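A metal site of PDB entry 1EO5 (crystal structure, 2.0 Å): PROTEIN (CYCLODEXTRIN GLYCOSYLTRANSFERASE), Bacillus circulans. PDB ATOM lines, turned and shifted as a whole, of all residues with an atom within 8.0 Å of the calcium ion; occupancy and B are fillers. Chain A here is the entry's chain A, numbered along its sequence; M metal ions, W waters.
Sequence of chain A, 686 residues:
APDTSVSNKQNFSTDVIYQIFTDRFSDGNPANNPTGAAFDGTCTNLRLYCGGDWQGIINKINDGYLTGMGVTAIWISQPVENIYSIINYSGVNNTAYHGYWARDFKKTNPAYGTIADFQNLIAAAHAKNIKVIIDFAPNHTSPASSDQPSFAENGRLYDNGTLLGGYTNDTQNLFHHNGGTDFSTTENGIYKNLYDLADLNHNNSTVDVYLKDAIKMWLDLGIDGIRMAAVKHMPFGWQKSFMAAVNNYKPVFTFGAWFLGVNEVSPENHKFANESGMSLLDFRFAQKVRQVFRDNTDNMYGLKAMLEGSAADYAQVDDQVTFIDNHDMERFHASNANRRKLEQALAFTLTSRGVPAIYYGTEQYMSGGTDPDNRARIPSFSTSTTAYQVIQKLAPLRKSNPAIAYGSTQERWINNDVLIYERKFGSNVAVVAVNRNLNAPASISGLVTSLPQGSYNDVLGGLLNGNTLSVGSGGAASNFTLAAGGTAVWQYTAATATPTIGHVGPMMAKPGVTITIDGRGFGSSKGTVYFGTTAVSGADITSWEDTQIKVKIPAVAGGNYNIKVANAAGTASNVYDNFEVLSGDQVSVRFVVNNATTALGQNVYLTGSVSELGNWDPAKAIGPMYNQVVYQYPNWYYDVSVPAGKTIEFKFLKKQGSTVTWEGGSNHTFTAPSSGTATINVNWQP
The side-chain amide nitrogen (ND2) of Asn 33 sits close to the backbone carbonyl oxygen (O) of Pro 30 (3.3 Å).
The side-chain carboxylate (OD1) of Asp 53 sits at hydrogen-bond distance from the backbone NH (N) of Gly 28, at 2.7 Å.
N of Asp 53 lies within hydrogen-bond range of O of Ser 26 (2.9 Å).
The side-chain carboxylate (OD1) of Asp 53 sits close to the backbone NH (N) of Gln 55.
The backbone NH (N) of Gly 56 lies within hydrogen-bond range of the side-chain carboxylate (OD1) of Asp 53 (2.9 Å).
The side-chain amide oxygen of Asn 32 lies close to the backbone carbonyl oxygen of Ala 111 (3.1 Å).
The side-chain carboxylate of Asp 23 sits at hydrogen-bond distance from the backbone NH of Gly 51 (2.9 Å).
OD1 of Asn 29 sits at hydrogen-bond distance from N of Ala 31, at 2.9 Å.
The calcium ion is bound by the side-chain amide oxygen (OD1) of Asn 33, the side-chain carboxylate (OD2) of Asp 53, the side-chain amide oxygen (OD1) of Asn 32, water W1, the side-chain carboxylate (OD1) of Asp 27, the backbone carbonyl oxygen (O) of Gly 51 and the backbone carbonyl oxygen (O) of Asn 29.
The calcium ion has seven donor atoms within binding distance.
The nearest printed residue that does not touch the calcium ion is Pro 30 (4.1 Å).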
ATOM      1  N   THR A  22     -13.744 -24.318 -23.408  1.00  0.00           N
ATOM      2  CA  THR A  22     -13.745 -23.547 -24.651  1.00  0.00           C
ATOM      3  C   THR A  22     -14.085 -22.057 -24.556  1.00  0.00           C
ATOM      4  O   THR A  22     -13.333 -21.212 -25.030  1.00  0.00           O
ATOM      5  CB  THR A  22     -14.583 -24.218 -25.739  1.00  0.00           C
ATOM      6  OG1 THR A  22     -14.209 -25.596 -25.858  1.00  0.00           O
ATOM      7  CG2 THR A  22     -14.371 -23.522 -27.082  1.00  0.00           C
ATOM      8  N   ASP A  23     -15.221 -21.747 -23.950  1.00  0.00           N
ATOM      9  CA  ASP A  23     -15.676 -20.367 -23.841  1.00  0.00           C
ATOM     10  C   ASP A  23     -14.687 -19.468 -23.096  1.00  0.00           C
ATOM     11  O   ASP A  23     -14.706 -18.248 -23.276  1.00  0.00           O
ATOM     12  CB  ASP A  23     -17.044 -20.311 -23.166  1.00  0.00           C
ATOM     13  CG  ASP A  23     -17.604 -18.904 -23.125  1.00  0.00           C
ATOM     14  OD1 ASP A  23     -17.829 -18.322 -24.208  1.00  0.00           O
ATOM     15  OD2 ASP A  23     -17.806 -18.363 -22.012  1.00  0.00           O
ATOM     16  N   SER A  26      -9.932 -18.882 -25.444  1.00  0.00           N
ATOM     17  CA  SER A  26      -9.531 -17.876 -26.426  1.00  0.00           C
ATOM     18  C   SER A  26     -10.608 -17.608 -27.472  1.00  0.00           C
ATOM     19  O   SER A  26     -10.950 -18.492 -28.259  1.00  0.00           O
ATOM     20  CB  SER A  26      -8.224 -18.291 -27.107  1.00  0.00           C
ATOM     21  OG  SER A  26      -7.797 -17.292 -28.019  1.00  0.00           O
ATOM     22  N   ASP A  27     -11.098 -16.378 -27.505  1.00  0.00           N
ATOM     23  CA  ASP A  27     -12.063 -15.982 -28.515  1.00  0.00           C
ATOM     24  C   ASP A  27     -11.306 -15.639 -29.787  1.00  0.00           C
ATOM     25  O   ASP A  27     -10.841 -14.515 -29.963  1.00  0.00           O
ATOM     26  CB  ASP A  27     -12.860 -14.762 -28.034  1.00  0.00           C
ATOM     27  CG  ASP A  27     -13.822 -14.235 -29.097  1.00  0.00           C
ATOM     28  OD1 ASP A  27     -13.975 -14.896 -30.149  1.00  0.00           O
ATOM     29  OD2 ASP A  27     -14.433 -13.171 -28.874  1.00  0.00           O
ATOM     30  N   GLY A  28     -11.143 -16.632 -30.647  1.00  0.00           N
ATOM     31  CA  GLY A  28     -10.404 -16.444 -31.887  1.00  0.00           C
ATOM     32  C   GLY A  28     -11.300 -15.859 -32.982  1.00  0.00           C
ATOM     33  O   GLY A  28     -10.810 -15.416 -34.020  1.00  0.00           O
ATOM     34  N   ASN A  29     -12.600 -15.891 -32.746  1.00  0.00           N
ATOM     35  CA  ASN A  29     -13.557 -15.386 -33.728  1.00  0.00           C
ATOM     36  C   ASN A  29     -14.710 -14.646 -33.085  1.00  0.00           C
ATOM     37  O   ASN A  29     -15.757 -15.224 -32.792  1.00  0.00           O
ATOM     38  CB  ASN A  29     -14.084 -16.519 -34.608  1.00  0.00           C
ATOM     39  CG  ASN A  29     -15.041 -16.032 -35.660  1.00  0.00           C
ATOM     40  OD1 ASN A  29     -15.215 -14.828 -35.850  1.00  0.00           O
ATOM     41  ND2 ASN A  29     -15.675 -16.966 -36.355  1.00  0.00           N
ATOM     42  N   PRO A  30     -14.540 -13.349 -32.888  1.00  0.00           N
ATOM     43  CA  PRO A  30     -15.582 -12.522 -32.279  1.00  0.00           C
ATOM     44  C   PRO A  30     -16.876 -12.597 -33.068  1.00  0.00           C
ATOM     45  O   PRO A  30     -17.967 -12.436 -32.513  1.00  0.00           O
ATOM     46  CB  PRO A  30     -14.994 -11.096 -32.357  1.00  0.00           C
ATOM     47  CG  PRO A  30     -13.529 -11.289 -32.657  1.00  0.00           C
ATOM     48  CD  PRO A  30     -13.444 -12.533 -33.441  1.00  0.00           C
ATOM     49  N   ALA A  31     -16.762 -12.844 -34.368  1.00  0.00           N
ATOM     50  CA  ALA A  31     -17.930 -12.909 -35.243  1.00  0.00           C
ATOM     51  C   ALA A  31     -18.953 -13.944 -34.775  1.00  0.00           C
ATOM     52  O   ALA A  31     -20.156 -13.774 -34.975  1.00  0.00           O
ATOM     53  CB  ALA A  31     -17.508 -13.180 -36.677  1.00  0.00           C
ATOM     54  N   ASN A  32     -18.486 -15.023 -34.150  1.00  0.00           N
ATOM     55  CA  ASN A  32     -19.393 -16.079 -33.702  1.00  0.00           C
ATOM     56  C   ASN A  32     -19.872 -15.927 -32.260  1.00  0.00           C
ATOM     57  O   ASN A  32     -20.592 -16.787 -31.748  1.00  0.00           O
ATOM     58  CB  ASN A  32     -18.789 -17.473 -33.934  1.00  0.00           C
ATOM     59  CG  ASN A  32     -17.538 -17.725 -33.113  1.00  0.00           C
ATOM     60  OD1 ASN A  32     -17.399 -17.212 -31.998  1.00  0.00           O
ATOM     61  ND2 ASN A  32     -16.638 -18.545 -33.631  1.00  0.00           N
ATOM     62  N   ASN A  33     -19.484 -14.836 -31.611  1.00  0.00           N
ATOM     63  CA  ASN A  33     -19.886 -14.599 -30.231  1.00  0.00           C
ATOM     64  C   ASN A  33     -21.402 -14.437 -30.092  1.00  0.00           C
ATOM     65  O   ASN A  33     -22.045 -13.872 -30.965  1.00  0.00           O
ATOM     66  CB  ASN A  33     -19.191 -13.361 -29.663  1.00  0.00           C
ATOM     67  CG  ASN A  33     -17.686 -13.513 -29.608  1.00  0.00           C
ATOM     68  OD1 ASN A  33     -17.158 -14.606 -29.812  1.00  0.00           O
ATOM     69  ND2 ASN A  33     -16.991 -12.422 -29.351  1.00  0.00           N
ATOM     70  N   PRO A  34     -21.947 -14.900 -28.975  1.00  0.00           N
ATOM     71  CA  PRO A  34     -23.354 -14.715 -28.681  1.00  0.00           C
ATOM     72  C   PRO A  34     -23.555 -13.231 -28.397  1.00  0.00           C
ATOM     73  O   PRO A  34     -22.596 -12.513 -28.125  1.00  0.00           O
ATOM     74  CB  PRO A  34     -23.558 -15.525 -27.415  1.00  0.00           C
ATOM     75  CG  PRO A  34     -22.580 -16.640 -27.533  1.00  0.00           C
ATOM     76  CD  PRO A  34     -21.387 -16.086 -28.281  1.00  0.00           C
ATOM     77  N   PHE A  39     -24.281 -12.577 -23.413  1.00  0.00           N
ATOM     78  CA  PHE A  39     -22.883 -12.291 -23.636  1.00  0.00           C
ATOM     79  C   PHE A  39     -22.262 -11.245 -22.712  1.00  0.00           C
ATOM     80  O   PHE A  39     -22.919 -10.296 -22.276  1.00  0.00           O
ATOM     81  CB  PHE A  39     -22.663 -11.893 -25.090  1.00  0.00           C
ATOM     82  CG  PHE A  39     -21.223 -11.769 -25.484  1.00  0.00           C
ATOM     83  CD1 PHE A  39     -20.419 -12.889 -25.616  1.00  0.00           C
ATOM     84  CD2 PHE A  39     -20.680 -10.526 -25.764  1.00  0.00           C
ATOM     85  CE1 PHE A  39     -19.100 -12.770 -25.998  1.00  0.00           C
ATOM     86  CE2 PHE A  39     -19.350 -10.403 -26.139  1.00  0.00           C
ATOM     87  CZ  PHE A  39     -18.566 -11.529 -26.263  1.00  0.00           C
ATOM     88  N   TYR A  49     -21.733 -16.185 -21.828  1.00  0.00           N
ATOM     89  CA  TYR A  49     -20.743 -16.538 -22.826  1.00  0.00           C
ATOM     90  C   TYR A  49     -19.680 -15.447 -22.855  1.00  0.00           C
ATOM     91  O   TYR A  49     -19.998 -14.260 -22.836  1.00  0.00           O
ATOM     92  CB  TYR A  49     -21.389 -16.653 -24.207  1.00  0.00           C
ATOM     93  CG  TYR A  49     -21.919 -18.030 -24.552  1.00  0.00           C
ATOM     94  CD1 TYR A  49     -21.106 -18.987 -25.139  1.00  0.00           C
ATOM     95  CD2 TYR A  49     -23.277 -18.319 -24.427  1.00  0.00           C
ATOM     96  CE1 TYR A  49     -21.599 -20.221 -25.513  1.00  0.00           C
ATOM     97  CE2 TYR A  49     -23.779 -19.552 -24.800  1.00  0.00           C
ATOM     98  CZ  TYR A  49     -22.939 -20.497 -25.341  1.00  0.00           C
ATOM     99  OH  TYR A  49     -23.441 -21.725 -25.705  1.00  0.00           O
ATOM    100  N   CYS A  50     -18.411 -15.846 -22.898  1.00  0.00           N
ATOM    101  CA  CYS A  50     -17.315 -14.878 -22.933  1.00  0.00           C
ATOM    102  C   CYS A  50     -16.701 -14.755 -24.322  1.00  0.00           C
ATOM    103  O   CYS A  50     -15.995 -13.788 -24.613  1.00  0.00           O
ATOM    104  CB  CYS A  50     -16.260 -15.229 -21.893  1.00  0.00           C
ATOM    105  SG  CYS A  50     -16.839 -15.113 -20.169  1.00  0.00           S
ATOM    106  N   GLY A  51     -16.991 -15.724 -25.186  1.00  0.00           N
ATOM    107  CA  GLY A  51     -16.549 -15.660 -26.581  1.00  0.00           C
ATOM    108  C   GLY A  51     -15.485 -16.689 -26.997  1.00  0.00           C
ATOM    109  O   GLY A  51     -15.193 -16.834 -28.177  1.00  0.00           O
ATOM    110  N   GLY A  52     -14.910 -17.383 -26.016  1.00  0.00           N
ATOM    111  CA  GLY A  52     -13.883 -18.403 -26.302  1.00  0.00           C
ATOM    112  C   GLY A  52     -14.408 -19.406 -27.338  1.00  0.00           C
ATOM    113  O   GLY A  52     -15.554 -19.822 -27.260  1.00  0.00           O
ATOM    114  N   ASP A  53     -13.567 -19.764 -28.306  1.00  0.00           N
ATOM    115  CA  ASP A  53     -14.018 -20.649 -29.388  1.00  0.00           C
ATOM    116  C   ASP A  53     -12.921 -21.536 -29.972  1.00  0.00           C
ATOM    117  O   ASP A  53     -11.768 -21.502 -29.531  1.00  0.00           O
ATOM    118  CB  ASP A  53     -14.679 -19.826 -30.497  1.00  0.00           C
ATOM    119  CG  ASP A  53     -13.805 -18.682 -30.978  1.00  0.00           C
ATOM    120  OD1 ASP A  53     -12.573 -18.876 -31.073  1.00  0.00           O
ATOM    121  OD2 ASP A  53     -14.346 -17.591 -31.236  1.00  0.00           O
ATOM    122  N   TRP A  54     -13.290 -22.323 -30.972  1.00  0.00           N
ATOM    123  CA  TRP A  54     -12.366 -23.266 -31.599  1.00  0.00           C
ATOM    124  C   TRP A  54     -11.238 -22.577 -32.365  1.00  0.00           C
ATOM    125  O   TRP A  54     -10.116 -23.087 -32.400  1.00  0.00           O
ATOM    126  CB  TRP A  54     -13.119 -24.265 -32.480  1.00  0.00           C
ATOM    127  CG  TRP A  54     -14.011 -25.169 -31.691  1.00  0.00           C
ATOM    128  CD1 TRP A  54     -13.856 -25.540 -30.378  1.00  0.00           C
ATOM    129  CD2 TRP A  54     -15.234 -25.776 -32.131  1.00  0.00           C
ATOM    130  NE1 TRP A  54     -14.895 -26.351 -29.988  1.00  0.00           N
ATOM    131  CE2 TRP A  54     -15.751 -26.516 -31.047  1.00  0.00           C
ATOM    132  CE3 TRP A  54     -15.930 -25.778 -33.346  1.00  0.00           C
ATOM    133  CZ2 TRP A  54     -16.936 -27.237 -31.138  1.00  0.00           C
ATOM    134  CZ3 TRP A  54     -17.104 -26.504 -33.424  1.00  0.00           C
ATOM    135  CH2 TRP A  54     -17.597 -27.220 -32.336  1.00  0.00           C
ATOM    136  N   GLN A  55     -11.528 -21.420 -32.950  1.00  0.00           N
ATOM    137  CA  GLN A  55     -10.495 -20.669 -33.642  1.00  0.00           C
ATOM    138  C   GLN A  55      -9.430 -20.273 -32.635  1.00  0.00           C
ATOM    139  O   GLN A  55      -8.233 -20.391 -32.883  1.00  0.00           O
ATOM    140  CB  GLN A  55     -11.066 -19.426 -34.320  1.00  0.00           C
ATOM    141  CG  GLN A  55     -10.056 -18.651 -35.173  1.00  0.00           C
ATOM    142  CD  GLN A  55      -9.429 -19.513 -36.259  1.00  0.00           C
ATOM    143  OE1 GLN A  55     -10.124 -20.043 -37.127  1.00  0.00           O
ATOM    144  NE2 GLN A  55      -8.106 -19.651 -36.227  1.00  0.00           N
ATOM    145  N   GLY A  56      -9.877 -19.867 -31.448  1.00  0.00           N
ATOM    146  CA  GLY A  56      -8.973 -19.517 -30.363  1.00  0.00           C
ATOM    147  C   GLY A  56      -8.033 -20.685 -30.061  1.00  0.00           C
ATOM    148  O   GLY A  56      -6.816 -20.509 -30.003  1.00  0.00           O
ATOM    149  N   PRO A 110     -22.745 -23.156 -32.302  1.00  0.00           N
ATOM    150  CA  PRO A 110     -22.287 -22.053 -33.151  1.00  0.00           C
ATOM    151  C   PRO A 110     -21.332 -21.064 -32.474  1.00  0.00           C
ATOM    152  O   PRO A 110     -20.524 -20.416 -33.137  1.00  0.00           O
ATOM    153  CB  PRO A 110     -23.587 -21.351 -33.567  1.00  0.00           C
ATOM    154  CG  PRO A 110     -24.661 -21.945 -32.690  1.00  0.00           C
ATOM    155  CD  PRO A 110     -24.208 -23.297 -32.336  1.00  0.00           C
ATOM    156  N   ALA A 111     -21.434 -20.957 -31.155  1.00  0.00           N
ATOM    157  CA  ALA A 111     -20.556 -20.065 -30.397  1.00  0.00           C
ATOM    158  C   ALA A 111     -19.125 -20.599 -30.450  1.00  0.00           C
ATOM    159  O   ALA A 111     -18.156 -19.829 -30.465  1.00  0.00           O
ATOM    160  CB  ALA A 111     -21.027 -19.928 -28.960  1.00  0.00           C
ATOM    161  N   TYR A 112     -18.998 -21.924 -30.473  1.00  0.00           N
ATOM    162  CA  TYR A 112     -17.687 -22.571 -30.557  1.00  0.00           C
ATOM    163  C   TYR A 112     -17.194 -22.557 -31.991  1.00  0.00           C
ATOM    164  O   TYR A 112     -16.003 -22.353 -32.247  1.00  0.00           O
ATOM    165  CB  TYR A 112     -17.772 -24.027 -30.061  1.00  0.00           C
ATOM    166  CG  TYR A 112     -18.129 -24.184 -28.593  1.00  0.00           C
ATOM    167  CD1 TYR A 112     -18.177 -23.081 -27.746  1.00  0.00           C
ATOM    168  CD2 TYR A 112     -18.415 -25.431 -28.064  1.00  0.00           C
ATOM    169  CE1 TYR A 112     -18.505 -23.223 -26.408  1.00  0.00           C
ATOM    170  CE2 TYR A 112     -18.755 -25.585 -26.729  1.00  0.00           C
ATOM    171  CZ  TYR A 112     -18.795 -24.484 -25.905  1.00  0.00           C
ATOM    172  OH  TYR A 112     -19.125 -24.636 -24.584  1.00  0.00           O
ATOM    173  N   GLY A 113     -18.106 -22.774 -32.929  1.00  0.00           N
ATOM    174  CA  GLY A 113     -17.772 -22.755 -34.338  1.00  0.00           C
ATOM    175  C   GLY A 113     -18.650 -23.674 -35.162  1.00  0.00           C
ATOM    176  O   GLY A 113     -19.582 -24.306 -34.649  1.00  0.00           O
HETATM  177 CA    CA M   1     -16.001 -16.255 -30.461  1.00  0.00          CA
HETATM  178  O   HOH W   1     -17.702 -17.376 -29.324  1.00  0.00           O
